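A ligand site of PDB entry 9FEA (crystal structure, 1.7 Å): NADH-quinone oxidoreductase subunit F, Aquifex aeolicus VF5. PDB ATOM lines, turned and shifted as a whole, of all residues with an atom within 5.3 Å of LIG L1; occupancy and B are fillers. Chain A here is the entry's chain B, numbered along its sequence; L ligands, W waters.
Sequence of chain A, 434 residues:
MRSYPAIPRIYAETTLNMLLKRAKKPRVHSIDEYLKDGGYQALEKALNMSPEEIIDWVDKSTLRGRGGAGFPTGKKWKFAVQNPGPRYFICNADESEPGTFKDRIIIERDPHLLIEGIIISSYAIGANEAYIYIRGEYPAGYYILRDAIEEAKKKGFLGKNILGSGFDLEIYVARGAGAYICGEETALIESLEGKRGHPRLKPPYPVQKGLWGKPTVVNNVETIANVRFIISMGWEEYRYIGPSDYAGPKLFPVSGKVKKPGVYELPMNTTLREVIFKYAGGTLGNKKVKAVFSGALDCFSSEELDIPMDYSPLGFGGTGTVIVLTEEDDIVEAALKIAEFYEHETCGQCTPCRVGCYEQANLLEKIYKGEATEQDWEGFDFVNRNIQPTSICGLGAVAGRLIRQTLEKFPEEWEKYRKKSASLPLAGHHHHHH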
ATOM      1  N   GLY A  65      15.978  22.183 -20.482  1.00  0.00           N
ATOM      2  CA  GLY A  65      17.081  22.376 -21.398  1.00  0.00           C
ATOM      3  C   GLY A  65      18.054  23.448 -20.917  1.00  0.00           C
ATOM      4  O   GLY A  65      17.628  24.535 -20.514  1.00  0.00           O
ATOM      5  N   ARG A  66      19.359  23.117 -20.972  1.00  0.00           N
ATOM      6  CA  ARG A  66      20.427  23.999 -20.507  1.00  0.00           C
ATOM      7  C   ARG A  66      21.058  24.785 -21.661  1.00  0.00           C
ATOM      8  O   ARG A  66      22.078  25.463 -21.466  1.00  0.00           O
ATOM      9  CB  ARG A  66      21.482  23.140 -19.816  1.00  0.00           C
ATOM     10  CG  ARG A  66      20.940  22.374 -18.621  1.00  0.00           C
ATOM     11  CD  ARG A  66      20.630  23.277 -17.445  1.00  0.00           C
ATOM     12  NE  ARG A  66      20.486  22.516 -16.202  1.00  0.00           N
ATOM     13  CZ  ARG A  66      19.395  22.286 -15.508  1.00  0.00           C
ATOM     14  NH1 ARG A  66      19.492  21.831 -14.276  1.00  0.00           N
ATOM     15  NH2 ARG A  66      18.194  22.603 -15.996  1.00  0.00           N
ATOM     16  N   GLY A  67      20.448  24.696 -22.845  1.00  0.00           N
ATOM     17  CA  GLY A  67      20.998  25.341 -24.030  1.00  0.00           C
ATOM     18  C   GLY A  67      20.478  26.763 -24.214  1.00  0.00           C
ATOM     19  O   GLY A  67      20.877  27.421 -25.184  1.00  0.00           O
ATOM     20  N   GLY A  68      19.608  27.234 -23.298  1.00  0.00           N
ATOM     21  CA  GLY A  68      19.203  28.629 -23.286  1.00  0.00           C
ATOM     22  C   GLY A  68      17.685  28.815 -23.243  1.00  0.00           C
ATOM     23  O   GLY A  68      17.201  29.853 -22.784  1.00  0.00           O
ATOM     24  N   ALA A  69      16.922  27.845 -23.744  1.00  0.00           N
ATOM     25  CA  ALA A  69      15.477  28.051 -23.881  1.00  0.00           C
ATOM     26  C   ALA A  69      14.700  27.426 -22.724  1.00  0.00           C
ATOM     27  O   ALA A  69      13.521  27.743 -22.576  1.00  0.00           O
ATOM     28  CB  ALA A  69      14.971  27.495 -25.177  1.00  0.00           C
ATOM     29  N   GLY A  70      15.308  26.480 -21.999  1.00  0.00           N
ATOM     30  CA  GLY A  70      14.667  25.919 -20.815  1.00  0.00           C
ATOM     31  C   GLY A  70      13.431  25.075 -21.119  1.00  0.00           C
ATOM     32  O   GLY A  70      12.529  25.007 -20.281  1.00  0.00           O
ATOM     33  N   PHE A  71      13.382  24.392 -22.268  1.00  0.00           N
ATOM     34  CA  PHE A  71      12.256  23.519 -22.578  1.00  0.00           C
ATOM     35  C   PHE A  71      12.322  22.230 -21.759  1.00  0.00           C
ATOM     36  O   PHE A  71      13.384  21.639 -21.605  1.00  0.00           O
ATOM     37  CB  PHE A  71      12.152  23.163 -24.055  1.00  0.00           C
ATOM     38  CG  PHE A  71      10.792  22.612 -24.439  1.00  0.00           C
ATOM     39  CD1 PHE A  71       9.750  23.460 -24.794  1.00  0.00           C
ATOM     40  CD2 PHE A  71      10.566  21.243 -24.500  1.00  0.00           C
ATOM     41  CE1 PHE A  71       8.501  22.957 -25.166  1.00  0.00           C
ATOM     42  CE2 PHE A  71       9.325  20.738 -24.877  1.00  0.00           C
ATOM     43  CZ  PHE A  71       8.300  21.605 -25.212  1.00  0.00           C
ATOM     44  N   THR A  73      12.785  18.683 -20.657  1.00  0.00           N
ATOM     45  CA  THR A  73      13.459  17.651 -21.429  1.00  0.00           C
ATOM     46  C   THR A  73      12.563  16.424 -21.621  1.00  0.00           C
ATOM     47  O   THR A  73      12.472  15.876 -22.727  1.00  0.00           O
ATOM     48  CB  THR A  73      14.751  17.297 -20.702  1.00  0.00           C
ATOM     49  OG1 THR A  73      15.517  18.482 -20.535  1.00  0.00           O
ATOM     50  CG2 THR A  73      15.555  16.264 -21.455  1.00  0.00           C
ATOM     51  N   LYS A  76       9.984  17.015 -24.217  1.00  0.00           N
ATOM     52  CA  LYS A  76      10.574  16.957 -25.545  1.00  0.00           C
ATOM     53  C   LYS A  76      10.691  15.501 -26.009  1.00  0.00           C
ATOM     54  O   LYS A  76      10.285  15.147 -27.127  1.00  0.00           O
ATOM     55  CB  LYS A  76      11.911  17.703 -25.552  1.00  0.00           C
ATOM     56  CG  LYS A  76      12.520  17.846 -26.950  1.00  0.00           C
ATOM     57  CD  LYS A  76      13.943  18.344 -26.972  1.00  0.00           C
ATOM     58  CE  LYS A  76      14.071  19.723 -26.413  1.00  0.00           C
ATOM     59  NZ  LYS A  76      15.424  20.234 -26.649  1.00  0.00           N
ATOM     60  N   ASN A  92      24.050  18.695 -28.686  1.00  0.00           N
ATOM     61  CA  ASN A  92      24.496  20.000 -29.139  1.00  0.00           C
ATOM     62  C   ASN A  92      25.693  20.464 -28.316  1.00  0.00           C
ATOM     63  O   ASN A  92      25.529  20.906 -27.186  1.00  0.00           O
ATOM     64  CB  ASN A  92      23.344  20.983 -29.056  1.00  0.00           C
ATOM     65  CG  ASN A  92      23.637  22.268 -29.791  1.00  0.00           C
ATOM     66  OD1 ASN A  92      24.796  22.650 -29.995  1.00  0.00           O
ATOM     67  ND2 ASN A  92      22.587  22.976 -30.156  1.00  0.00           N
ATOM     68  N   ASP A  94      27.827  22.879 -29.614  1.00  0.00           N
ATOM     69  CA  ASP A  94      28.298  23.973 -30.444  1.00  0.00           C
ATOM     70  C   ASP A  94      28.737  25.187 -29.619  1.00  0.00           C
ATOM     71  O   ASP A  94      29.362  26.077 -30.192  1.00  0.00           O
ATOM     72  CB  ASP A  94      27.299  24.426 -31.501  1.00  0.00           C
ATOM     73  CG  ASP A  94      27.965  25.158 -32.659  1.00  0.00           C
ATOM     74  OD1 ASP A  94      28.800  24.527 -33.331  1.00  0.00           O
ATOM     75  OD2 ASP A  94      27.724  26.398 -32.816  1.00  0.00           O
ATOM     76  N   GLU A  95      28.398  25.232 -28.323  1.00  0.00           N
ATOM     77  CA  GLU A  95      28.722  26.296 -27.385  1.00  0.00           C
ATOM     78  C   GLU A  95      29.622  27.411 -27.967  1.00  0.00           C
ATOM     79  O   GLU A  95      30.843  27.322 -27.904  1.00  0.00           O
ATOM     80  CB  GLU A  95      29.411  25.675 -26.180  1.00  0.00           C
ATOM     81  CG  GLU A  95      29.820  26.700 -25.110  1.00  0.00           C
ATOM     82  CD  GLU A  95      30.217  26.024 -23.824  1.00  0.00           C
ATOM     83  OE1 GLU A  95      31.332  25.416 -23.735  1.00  0.00           O
ATOM     84  OE2 GLU A  95      29.397  26.089 -22.895  1.00  0.00           O
ATOM     85  N   SER A  96      29.011  28.485 -28.484  1.00  0.00           N
ATOM     86  CA  SER A  96      29.712  29.595 -29.099  1.00  0.00           C
ATOM     87  C   SER A  96      29.206  30.982 -28.669  1.00  0.00           C
ATOM     88  O   SER A  96      29.642  31.965 -29.231  1.00  0.00           O
ATOM     89  CB  SER A  96      29.631  29.469 -30.611  1.00  0.00           C
ATOM     90  OG  SER A  96      30.466  28.392 -31.008  1.00  0.00           O
ATOM     91  N   ASP A 103      30.036  24.007 -21.163  1.00  0.00           N
ATOM     92  CA  ASP A 103      29.889  22.691 -21.773  1.00  0.00           C
ATOM     93  C   ASP A 103      31.249  22.044 -21.989  1.00  0.00           C
ATOM     94  O   ASP A 103      31.383  20.821 -21.876  1.00  0.00           O
ATOM     95  CB  ASP A 103      29.084  22.736 -23.045  1.00  0.00           C
ATOM     96  CG  ASP A 103      27.656  23.213 -22.888  1.00  0.00           C
ATOM     97  OD1 ASP A 103      27.157  23.149 -21.723  1.00  0.00           O
ATOM     98  OD2 ASP A 103      27.080  23.635 -23.922  1.00  0.00           O
ATOM     99  N   TYR A 180      28.349  30.430 -35.395  1.00  0.00           N
ATOM    100  CA  TYR A 180      27.550  30.399 -34.187  1.00  0.00           C
ATOM    101  C   TYR A 180      26.126  29.882 -34.433  1.00  0.00           C
ATOM    102  O   TYR A 180      25.557  29.216 -33.565  1.00  0.00           O
ATOM    103  CB  TYR A 180      27.473  31.808 -33.604  1.00  0.00           C
ATOM    104  CG  TYR A 180      26.425  32.012 -32.528  1.00  0.00           C
ATOM    105  CD1 TYR A 180      26.565  31.445 -31.268  1.00  0.00           C
ATOM    106  CD2 TYR A 180      25.334  32.833 -32.760  1.00  0.00           C
ATOM    107  CE1 TYR A 180      25.632  31.660 -30.278  1.00  0.00           C
ATOM    108  CE2 TYR A 180      24.398  33.054 -31.778  1.00  0.00           C
ATOM    109  CZ  TYR A 180      24.551  32.476 -30.532  1.00  0.00           C
ATOM    110  OH  TYR A 180      23.597  32.708 -29.600  1.00  0.00           O
ATOM    111  N   ILE A 181      25.599  30.142 -35.629  1.00  0.00           N
ATOM    112  CA  ILE A 181      24.228  29.819 -35.966  1.00  0.00           C
ATOM    113  C   ILE A 181      24.055  28.308 -35.974  1.00  0.00           C
ATOM    114  O   ILE A 181      22.938  27.843 -35.772  1.00  0.00           O
ATOM    115  CB  ILE A 181      23.779  30.481 -37.293  1.00  0.00           C
ATOM    116  CG1 ILE A 181      22.280  30.442 -37.500  1.00  0.00           C
ATOM    117  CG2 ILE A 181      24.490  29.877 -38.506  1.00  0.00           C
ATOM    118  CD1 ILE A 181      21.481  31.009 -36.342  1.00  0.00           C
ATOM    119  N   GLY A 183      24.675  26.348 -33.749  1.00  0.00           N
ATOM    120  CA  GLY A 183      24.119  25.946 -32.455  1.00  0.00           C
ATOM    121  C   GLY A 183      22.600  25.977 -32.424  1.00  0.00           C
ATOM    122  O   GLY A 183      21.981  25.329 -31.586  1.00  0.00           O
ATOM    123  N   GLU A 184      21.989  26.715 -33.361  1.00  0.00           N
ATOM    124  CA  GLU A 184      20.538  26.674 -33.471  1.00  0.00           C
ATOM    125  C   GLU A 184      20.187  25.283 -34.002  1.00  0.00           C
ATOM    126  O   GLU A 184      20.752  24.852 -35.001  1.00  0.00           O
ATOM    127  CB  GLU A 184      20.054  27.768 -34.407  1.00  0.00           C
ATOM    128  CG  GLU A 184      18.546  27.998 -34.363  1.00  0.00           C
ATOM    129  CD  GLU A 184      17.703  27.003 -35.141  1.00  0.00           C
ATOM    130  OE1 GLU A 184      18.238  26.453 -36.096  1.00  0.00           O
ATOM    131  OE2 GLU A 184      16.563  26.732 -34.766  1.00  0.00           O
ATOM    132  N   GLU A 185      19.264  24.596 -33.336  1.00  0.00           N
ATOM    133  CA  GLU A 185      19.099  23.163 -33.569  1.00  0.00           C
ATOM    134  C   GLU A 185      18.824  22.817 -35.039  1.00  0.00           C
ATOM    135  O   GLU A 185      19.291  21.783 -35.488  1.00  0.00           O
ATOM    136  CB  GLU A 185      18.035  22.567 -32.658  1.00  0.00           C
ATOM    137  CG  GLU A 185      16.657  23.158 -32.881  1.00  0.00           C
ATOM    138  CD  GLU A 185      15.575  22.648 -31.950  1.00  0.00           C
ATOM    139  OE1 GLU A 185      15.871  21.747 -31.127  1.00  0.00           O
ATOM    140  OE2 GLU A 185      14.467  23.196 -32.048  1.00  0.00           O
ATOM    141  N   LYS A 202      10.251  26.905 -38.018  1.00  0.00           N
ATOM    142  CA  LYS A 202       9.757  26.074 -36.936  1.00  0.00           C
ATOM    143  C   LYS A 202       8.446  26.678 -36.452  1.00  0.00           C
ATOM    144  O   LYS A 202       8.364  27.896 -36.324  1.00  0.00           O
ATOM    145  CB  LYS A 202      10.641  26.027 -35.689  1.00  0.00           C
ATOM    146  CG  LYS A 202      11.983  25.365 -35.813  1.00  0.00           C
ATOM    147  CD  LYS A 202      12.612  25.006 -34.459  1.00  0.00           C
ATOM    148  CE  LYS A 202      12.856  26.151 -33.502  1.00  0.00           C
ATOM    149  NZ  LYS A 202      14.039  25.934 -32.646  1.00  0.00           N
ATOM    150  N   VAL A 218      17.208  17.077 -30.113  1.00  0.00           N
ATOM    151  CA  VAL A 218      18.419  17.824 -29.859  1.00  0.00           C
ATOM    152  C   VAL A 218      18.412  18.255 -28.393  1.00  0.00           C
ATOM    153  O   VAL A 218      17.463  18.878 -27.943  1.00  0.00           O
ATOM    154  CB  VAL A 218      18.524  19.062 -30.770  1.00  0.00           C
ATOM    155  CG1 VAL A 218      19.844  19.778 -30.563  1.00  0.00           C
ATOM    156  CG2 VAL A 218      18.325  18.694 -32.225  1.00  0.00           C
ATOM    157  N   ASN A 219      19.497  17.943 -27.685  1.00  0.00           N
ATOM    158  CA  ASN A 219      19.704  18.439 -26.337  1.00  0.00           C
ATOM    159  C   ASN A 219      21.135  18.935 -26.150  1.00  0.00           C
ATOM    160  O   ASN A 219      22.063  18.425 -26.745  1.00  0.00           O
ATOM    161  CB  ASN A 219      19.407  17.395 -25.254  1.00  0.00           C
ATOM    162  CG  ASN A 219      17.936  17.299 -24.913  1.00  0.00           C
ATOM    163  OD1 ASN A 219      17.316  18.285 -24.484  1.00  0.00           O
ATOM    164  ND2 ASN A 219      17.395  16.103 -25.018  1.00  0.00           N
ATOM    165  N   ASN A 220      21.269  19.953 -25.294  1.00  0.00           N
ATOM    166  CA  ASN A 220      22.551  20.546 -24.935  1.00  0.00           C
ATOM    167  C   ASN A 220      23.380  19.586 -24.096  1.00  0.00           C
ATOM    168  O   ASN A 220      22.825  18.786 -23.338  1.00  0.00           O
ATOM    169  CB  ASN A 220      22.269  21.871 -24.254  1.00  0.00           C
ATOM    170  CG  ASN A 220      23.509  22.524 -23.709  1.00  0.00           C
ATOM    171  OD1 ASN A 220      24.290  23.136 -24.448  1.00  0.00           O
ATOM    172  ND2 ASN A 220      23.683  22.374 -22.426  1.00  0.00           N
ATOM    173  N   VAL A 221      24.712  19.710 -24.190  1.00  0.00           N
ATOM    174  CA  VAL A 221      25.666  18.919 -23.413  1.00  0.00           C
ATOM    175  C   VAL A 221      25.296  18.865 -21.924  1.00  0.00           C
ATOM    176  O   VAL A 221      25.210  17.795 -21.323  1.00  0.00           O
ATOM    177  CB  VAL A 221      27.075  19.519 -23.566  1.00  0.00           C
ATOM    178  CG1 VAL A 221      28.030  19.001 -22.485  1.00  0.00           C
ATOM    179  CG2 VAL A 221      27.624  19.239 -24.952  1.00  0.00           C
ATOM    180  N   THR A 223      22.456  19.562 -20.415  1.00  0.00           N
ATOM    181  CA  THR A 223      21.202  18.856 -20.188  1.00  0.00           C
ATOM    182  C   THR A 223      21.467  17.364 -20.048  1.00  0.00           C
ATOM    183  O   THR A 223      20.985  16.725 -19.105  1.00  0.00           O
ATOM    184  CB  THR A 223      20.225  19.097 -21.337  1.00  0.00           C
ATOM    185  OG1 THR A 223      20.132  20.498 -21.613  1.00  0.00           O
ATOM    186  CG2 THR A 223      18.849  18.546 -21.027  1.00  0.00           C
ATOM    187  N   CYS A 393      14.518  32.596 -36.804  1.00  0.00           N
ATOM    188  CA  CYS A 393      15.174  31.989 -35.639  1.00  0.00           C
ATOM    189  C   CYS A 393      15.481  33.013 -34.563  1.00  0.00           C
ATOM    190  O   CYS A 393      15.274  34.203 -34.707  1.00  0.00           O
ATOM    191  CB  CYS A 393      16.423  31.196 -36.011  1.00  0.00           C
ATOM    192  SG  CYS A 393      17.962  32.143 -35.983  1.00  0.00           S
ATOM    193  N   GLY A 394      15.936  32.515 -33.410  1.00  0.00           N
ATOM    194  CA  GLY A 394      16.128  33.357 -32.231  1.00  0.00           C
ATOM    195  C   GLY A 394      17.226  34.411 -32.374  1.00  0.00           C
ATOM    196  O   GLY A 394      17.220  35.363 -31.611  1.00  0.00           O
ATOM    197  N   LEU A 395      18.133  34.292 -33.358  1.00  0.00           N
ATOM    198  CA  LEU A 395      19.213  35.229 -33.475  1.00  0.00           C
ATOM    199  C   LEU A 395      18.632  36.595 -33.821  1.00  0.00           C
ATOM    200  O   LEU A 395      18.945  37.579 -33.168  1.00  0.00           O
ATOM    201  CB  LEU A 395      20.290  34.794 -34.473  1.00  0.00           C
ATOM    202  CG  LEU A 395      21.576  35.625 -34.472  1.00  0.00           C
ATOM    203  CD1 LEU A 395      22.758  34.799 -34.904  1.00  0.00           C
ATOM    204  CD2 LEU A 395      21.477  36.875 -35.372  1.00  0.00           C
HETATM  205  C1  LIG L   1      20.929  28.135 -29.904  1.00  0.00           C
HETATM  206  N1  LIG L   1      20.855  26.998 -29.050  1.00  0.00           N
HETATM  207  C2  LIG L   1      22.031  26.407 -28.654  1.00  0.00           C
HETATM  208  N2  LIG L   1      21.926  25.251 -27.922  1.00  0.00           N
HETATM  209  C3  LIG L   1      23.028  24.556 -27.516  1.00  0.00           C
HETATM  210  O1  LIG L   1      22.914  23.478 -26.921  1.00  0.00           O
HETATM  211  N3  LIG L   1      24.236  25.073 -27.855  1.00  0.00           N
HETATM  212  C4  LIG L   1      24.469  26.207 -28.624  1.00  0.00           C
HETATM  213  O2  LIG L   1      25.613  26.514 -28.906  1.00  0.00           O
HETATM  214  C5  LIG L   1      23.259  26.883 -29.006  1.00  0.00           C
HETATM  215  N4  LIG L   1      23.358  27.972 -29.842  1.00  0.00           N
HETATM  216  C6  LIG L   1      22.196  28.591 -30.304  1.00  0.00           C
HETATM  217  C7  LIG L   1      22.301  29.698 -31.155  1.00  0.00           C
HETATM  218  C8  LIG L   1      21.147  30.333 -31.608  1.00  0.00           C
HETATM  219  C9  LIG L   1      21.279  31.555 -32.491  1.00  0.00           C
HETATM  220  C10 LIG L   1      19.884  29.871 -31.201  1.00  0.00           C
HETATM  221  C11 LIG L   1      18.619  30.575 -31.605  1.00  0.00           C
HETATM  222  C12 LIG L   1      19.775  28.770 -30.358  1.00  0.00           C
HETATM  223  C13 LIG L   1      19.569  26.424 -28.666  1.00  0.00           C
HETATM  224  C14 LIG L   1      19.184  25.237 -29.549  1.00  0.00           C
HETATM  225  O3  LIG L   1      18.524  25.727 -30.721  1.00  0.00           O
HETATM  226  C15 LIG L   1      18.271  24.281 -28.784  1.00  0.00           C
HETATM  227  O4  LIG L   1      17.243  24.953 -28.071  1.00  0.00           O
HETATM  228  C16 LIG L   1      18.974  23.409 -27.752  1.00  0.00           C
HETATM  229  O5  LIG L   1      20.174  22.862 -28.260  1.00  0.00           O
HETATM  230  C17 LIG L   1      18.011  22.358 -27.253  1.00  0.00           C
HETATM  231  O6  LIG L   1      18.643  21.614 -26.182  1.00  0.00           O
HETATM  232  P1  LIG L   1      18.115  21.777 -24.668  1.00  0.00           P
HETATM  233  O7  LIG L   1      16.620  21.595 -24.610  1.00  0.00           O
HETATM  234  O8  LIG L   1      18.867  20.696 -23.899  1.00  0.00           O
HETATM  235  O9  LIG L   1      18.522  23.170 -24.241  1.00  0.00           O
HETATM  236  P1  LG2 L   2      12.748  27.286 -28.555  1.00  0.00           P
HETATM  237  O1  LG2 L   2      12.141  27.932 -27.358  1.00  0.00           O
HETATM  238  O2  LG2 L   2      12.089  27.426 -29.890  1.00  0.00           O
HETATM  239  O3  LG2 L   2      12.892  25.709 -28.277  1.00  0.00           O
HETATM  240  C1  LG2 L   2      13.726  25.152 -27.264  1.00  0.00           C
HETATM  241  C2  LG2 L   2      13.773  23.652 -27.459  1.00  0.00           C
HETATM  242  O4  LG2 L   2      12.445  23.111 -27.191  1.00  0.00           O
HETATM  243  C3  LG2 L   2      14.112  23.186 -28.877  1.00  0.00           C
HETATM  244  O5  LG2 L   2      14.759  21.921 -28.901  1.00  0.00           O
HETATM  245  C4  LG2 L   2      12.721  23.077 -29.525  1.00  0.00           C
HETATM  246  O6  LG2 L   2      12.711  22.189 -30.607  1.00  0.00           O
HETATM  247  C5  LG2 L   2      11.907  22.542 -28.361  1.00  0.00           C
HETATM  248  N1  LG2 L   2      10.483  22.887 -28.428  1.00  0.00           N
HETATM  249  C6  LG2 L   2       9.892  24.094 -28.138  1.00  0.00           C
HETATM  250  N2  LG2 L   2       8.593  24.080 -28.258  1.00  0.00           N
HETATM  251  C7  LG2 L   2       8.299  22.780 -28.665  1.00  0.00           C
HETATM  252  C8  LG2 L   2       7.082  22.147 -28.964  1.00  0.00           C
HETATM  253  N3  LG2 L   2       5.897  22.744 -28.894  1.00  0.00           N
HETATM  254  N4  LG2 L   2       7.141  20.836 -29.315  1.00  0.00           N
HETATM  255  C9  LG2 L   2       8.343  20.239 -29.378  1.00  0.00           C
HETATM  256  N5  LG2 L   2       9.544  20.744 -29.104  1.00  0.00           N
HETATM  257  C10 LG2 L   2       9.453  22.040 -28.763  1.00  0.00           C
HETATM  258  O7  LG2 L   2      14.229  27.866 -28.623  1.00  0.00           O
HETATM  259  P2  LG2 L   2      15.445  27.912 -29.677  1.00  0.00           P
HETATM  260  O8  LG2 L   2      14.969  28.577 -30.935  1.00  0.00           O
HETATM  261  O9  LG2 L   2      15.988  26.525 -29.815  1.00  0.00           O
HETATM  262  O10 LG2 L   2      16.520  28.838 -28.926  1.00  0.00           O
HETATM  263  C11 LG2 L   2      16.209  30.231 -28.623  1.00  0.00           C
HETATM  264  C12 LG2 L   2      16.195  30.415 -27.130  1.00  0.00           C
HETATM  265  O11 LG2 L   2      17.159  29.516 -26.535  1.00  0.00           O
HETATM  266  C13 LG2 L   2      16.607  31.796 -26.594  1.00  0.00           C
HETATM  267  O12 LG2 L   2      16.048  31.991 -25.296  1.00  0.00           O
HETATM  268  C14 LG2 L   2      18.142  31.687 -26.611  1.00  0.00           C
HETATM  269  O13 LG2 L   2      18.803  32.487 -25.643  1.00  0.00           O
HETATM  270  C15 LG2 L   2      18.366  30.216 -26.235  1.00  0.00           C
HETATM  271  N6  LG2 L   2      19.469  29.508 -26.930  1.00  0.00           N
HETATM  272  O   HOH W   1      26.490  28.085 -31.144  1.00  0.00           O
HETATM  273  O   HOH W   2      15.230  20.026 -22.979  1.00  0.00           O
HETATM  274  O   HOH W   3      23.647  30.598 -27.737  1.00  0.00           O
HETATM  275  O   HOH W   4      15.318  23.947 -24.265  1.00  0.00           O
HETATM  276  O   HOH W   5      26.148  28.979 -27.767  1.00  0.00           O
HETATM  277  O   HOH W   6      26.477  23.497 -26.614  1.00  0.00           O
HETATM  278  O   HOH W   7      23.092  28.548 -26.126  1.00  0.00           O
HETATM  279  O   HOH W   8      17.548  25.418 -25.191  1.00  0.00           O
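OD1 of Asn 220 lies close to OD2 of Asp 103. OE2 of Glu 185 lies within salt-bridge range of NZ of Lys 202. The side-chain amide oxygen of Asn 92 is in hydrogen-bond range of the backbone NH of Asp 94, at 3.1 Å. N of Gly 65 lies within hydrogen-bond range of O of Phe 71. N of Gly 70 lies close to O of Gly 65 (3.4 Å). The backbone carbonyl oxygen (O) of Asp 94 sits at hydrogen-bond distance from the side-chain hydroxyl (OG) of Ser 96, 2.7 Å away. The side-chain amino group (NZ) of Lys 202 lies within salt-bridge range of the side-chain carboxylate (OE2) of Glu 184 (3.4 Å). The side-chain sulfur of Cys 393 lies close to the backbone NH of Leu 395 (3.4 Å).
An oxygen (O8) of LIG L1 lies within hydrogen-bond range of the side-chain hydroxyl (OG1) of Thr 223. The side-chain amino group of Lys 76 is in salt-bridge range of an oxygen (O7) of LIG L1 (2.7 Å). N of Gly 67 lies within hydrogen-bond range of O9 of LIG L1. N of Asn 220 is in hydrogen-bond range of O8 of LIG L1 (2.9 Å). An oxygen (O1) of LIG L1 sits close to the side-chain amide oxygen (OD1) of Asn 220 (2.9 Å). An oxygen (O8) of LIG L1 sits close to the side-chain amide oxygen (OD1) of Asn 219. N of Glu 185 lies within hydrogen-bond range of O3 of LIG L1 (2.9 Å). The side-chain amide nitrogen (ND2) of Asn 92 sits at hydrogen-bond distance from an oxygen (O5) of LIG L1. O2 of LIG L1 sits at hydrogen-bond distance from N of Glu 95 (3.1 Å). N4 of LIG L1 sits close to O of Gly 183, at 3.5 Å. The backbone NH (N) of Arg 66 sits at hydrogen-bond distance from an oxygen (O9) of LIG L1, 3.4 Å away. The side-chain amino group (NZ) of Lys 76 lies within hydrogen-bond range of an oxygen (O5) of LG2 L2. The side-chain carboxylate (OE2) of Glu 185 lies within hydrogen-bond range of an oxygen (O6) of LG2 L2 (2.5 Å). The backbone carbonyl oxygen of Gly 68 sits at hydrogen-bond distance from an oxygen (O12) of LG2 L2, 3.5 Å away. N of Ala 69 is in hydrogen-bond range of O11 of LG2 L2 (3.3 Å). NZ of Lys 202 lies within salt-bridge range of O8 of LG2 L2 (3.3 Å).
The backbone carbonyl oxygen (O) of Val 218 lies close to an oxygen (O6) of LIG L1. Merely in contact with LIG L1: Gly 65 (3.3 Å), Asp 94 (3.5 Å), Ser 96 (3.95 Å), Tyr 180 (3.5 Å), Ile 181 (3.9 Å), Glu 184 (3.5 Å), Gly 394 (3.8 Å) and Leu 395 (3.9 Å). Hydrophobic or aromatic side chains that line LIG L1: Tyr 180, Ile 181, Val 218 and Leu 395. The nearest printed residue that does not touch LIG L1 is Gly 68 (4.3 Å).
An oxygen (O4) of LIG L1 is in hydrogen-bond range of an oxygen (O9) of LG2 L2.
Water W8 lies within hydrogen-bond range of O9 of LIG L1 (2.6 Å), N of Ala 69 (2.9 Å) and N of Gly 68 (3.3 Å). Water W2 lies within hydrogen-bond range of an oxygen (O7) of LIG L1 (2.7 Å), the backbone carbonyl oxygen of Phe 71 (2.8 Å), the side-chain hydroxyl of Thr 73 (2.9 Å), the side-chain amide oxygen of Asn 219 (3.1 Å) and the backbone NH of Gly 65 (3.4 Å). Water W4 lies within hydrogen-bond range of an oxygen (O7) of LIG L1, the backbone NH (N) of Phe 71 and the backbone NH (N) of Gly 70. Water W5 lies within hydrogen-bond range of an oxygen (O2) of LIG L1 (2.8 Å) and the backbone NH of Ser 96 (3.0 Å). Water W3 lies within hydrogen-bond range of the side-chain hydroxyl (OH) of Tyr 180 and a nitrogen (N4) of LIG L1.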
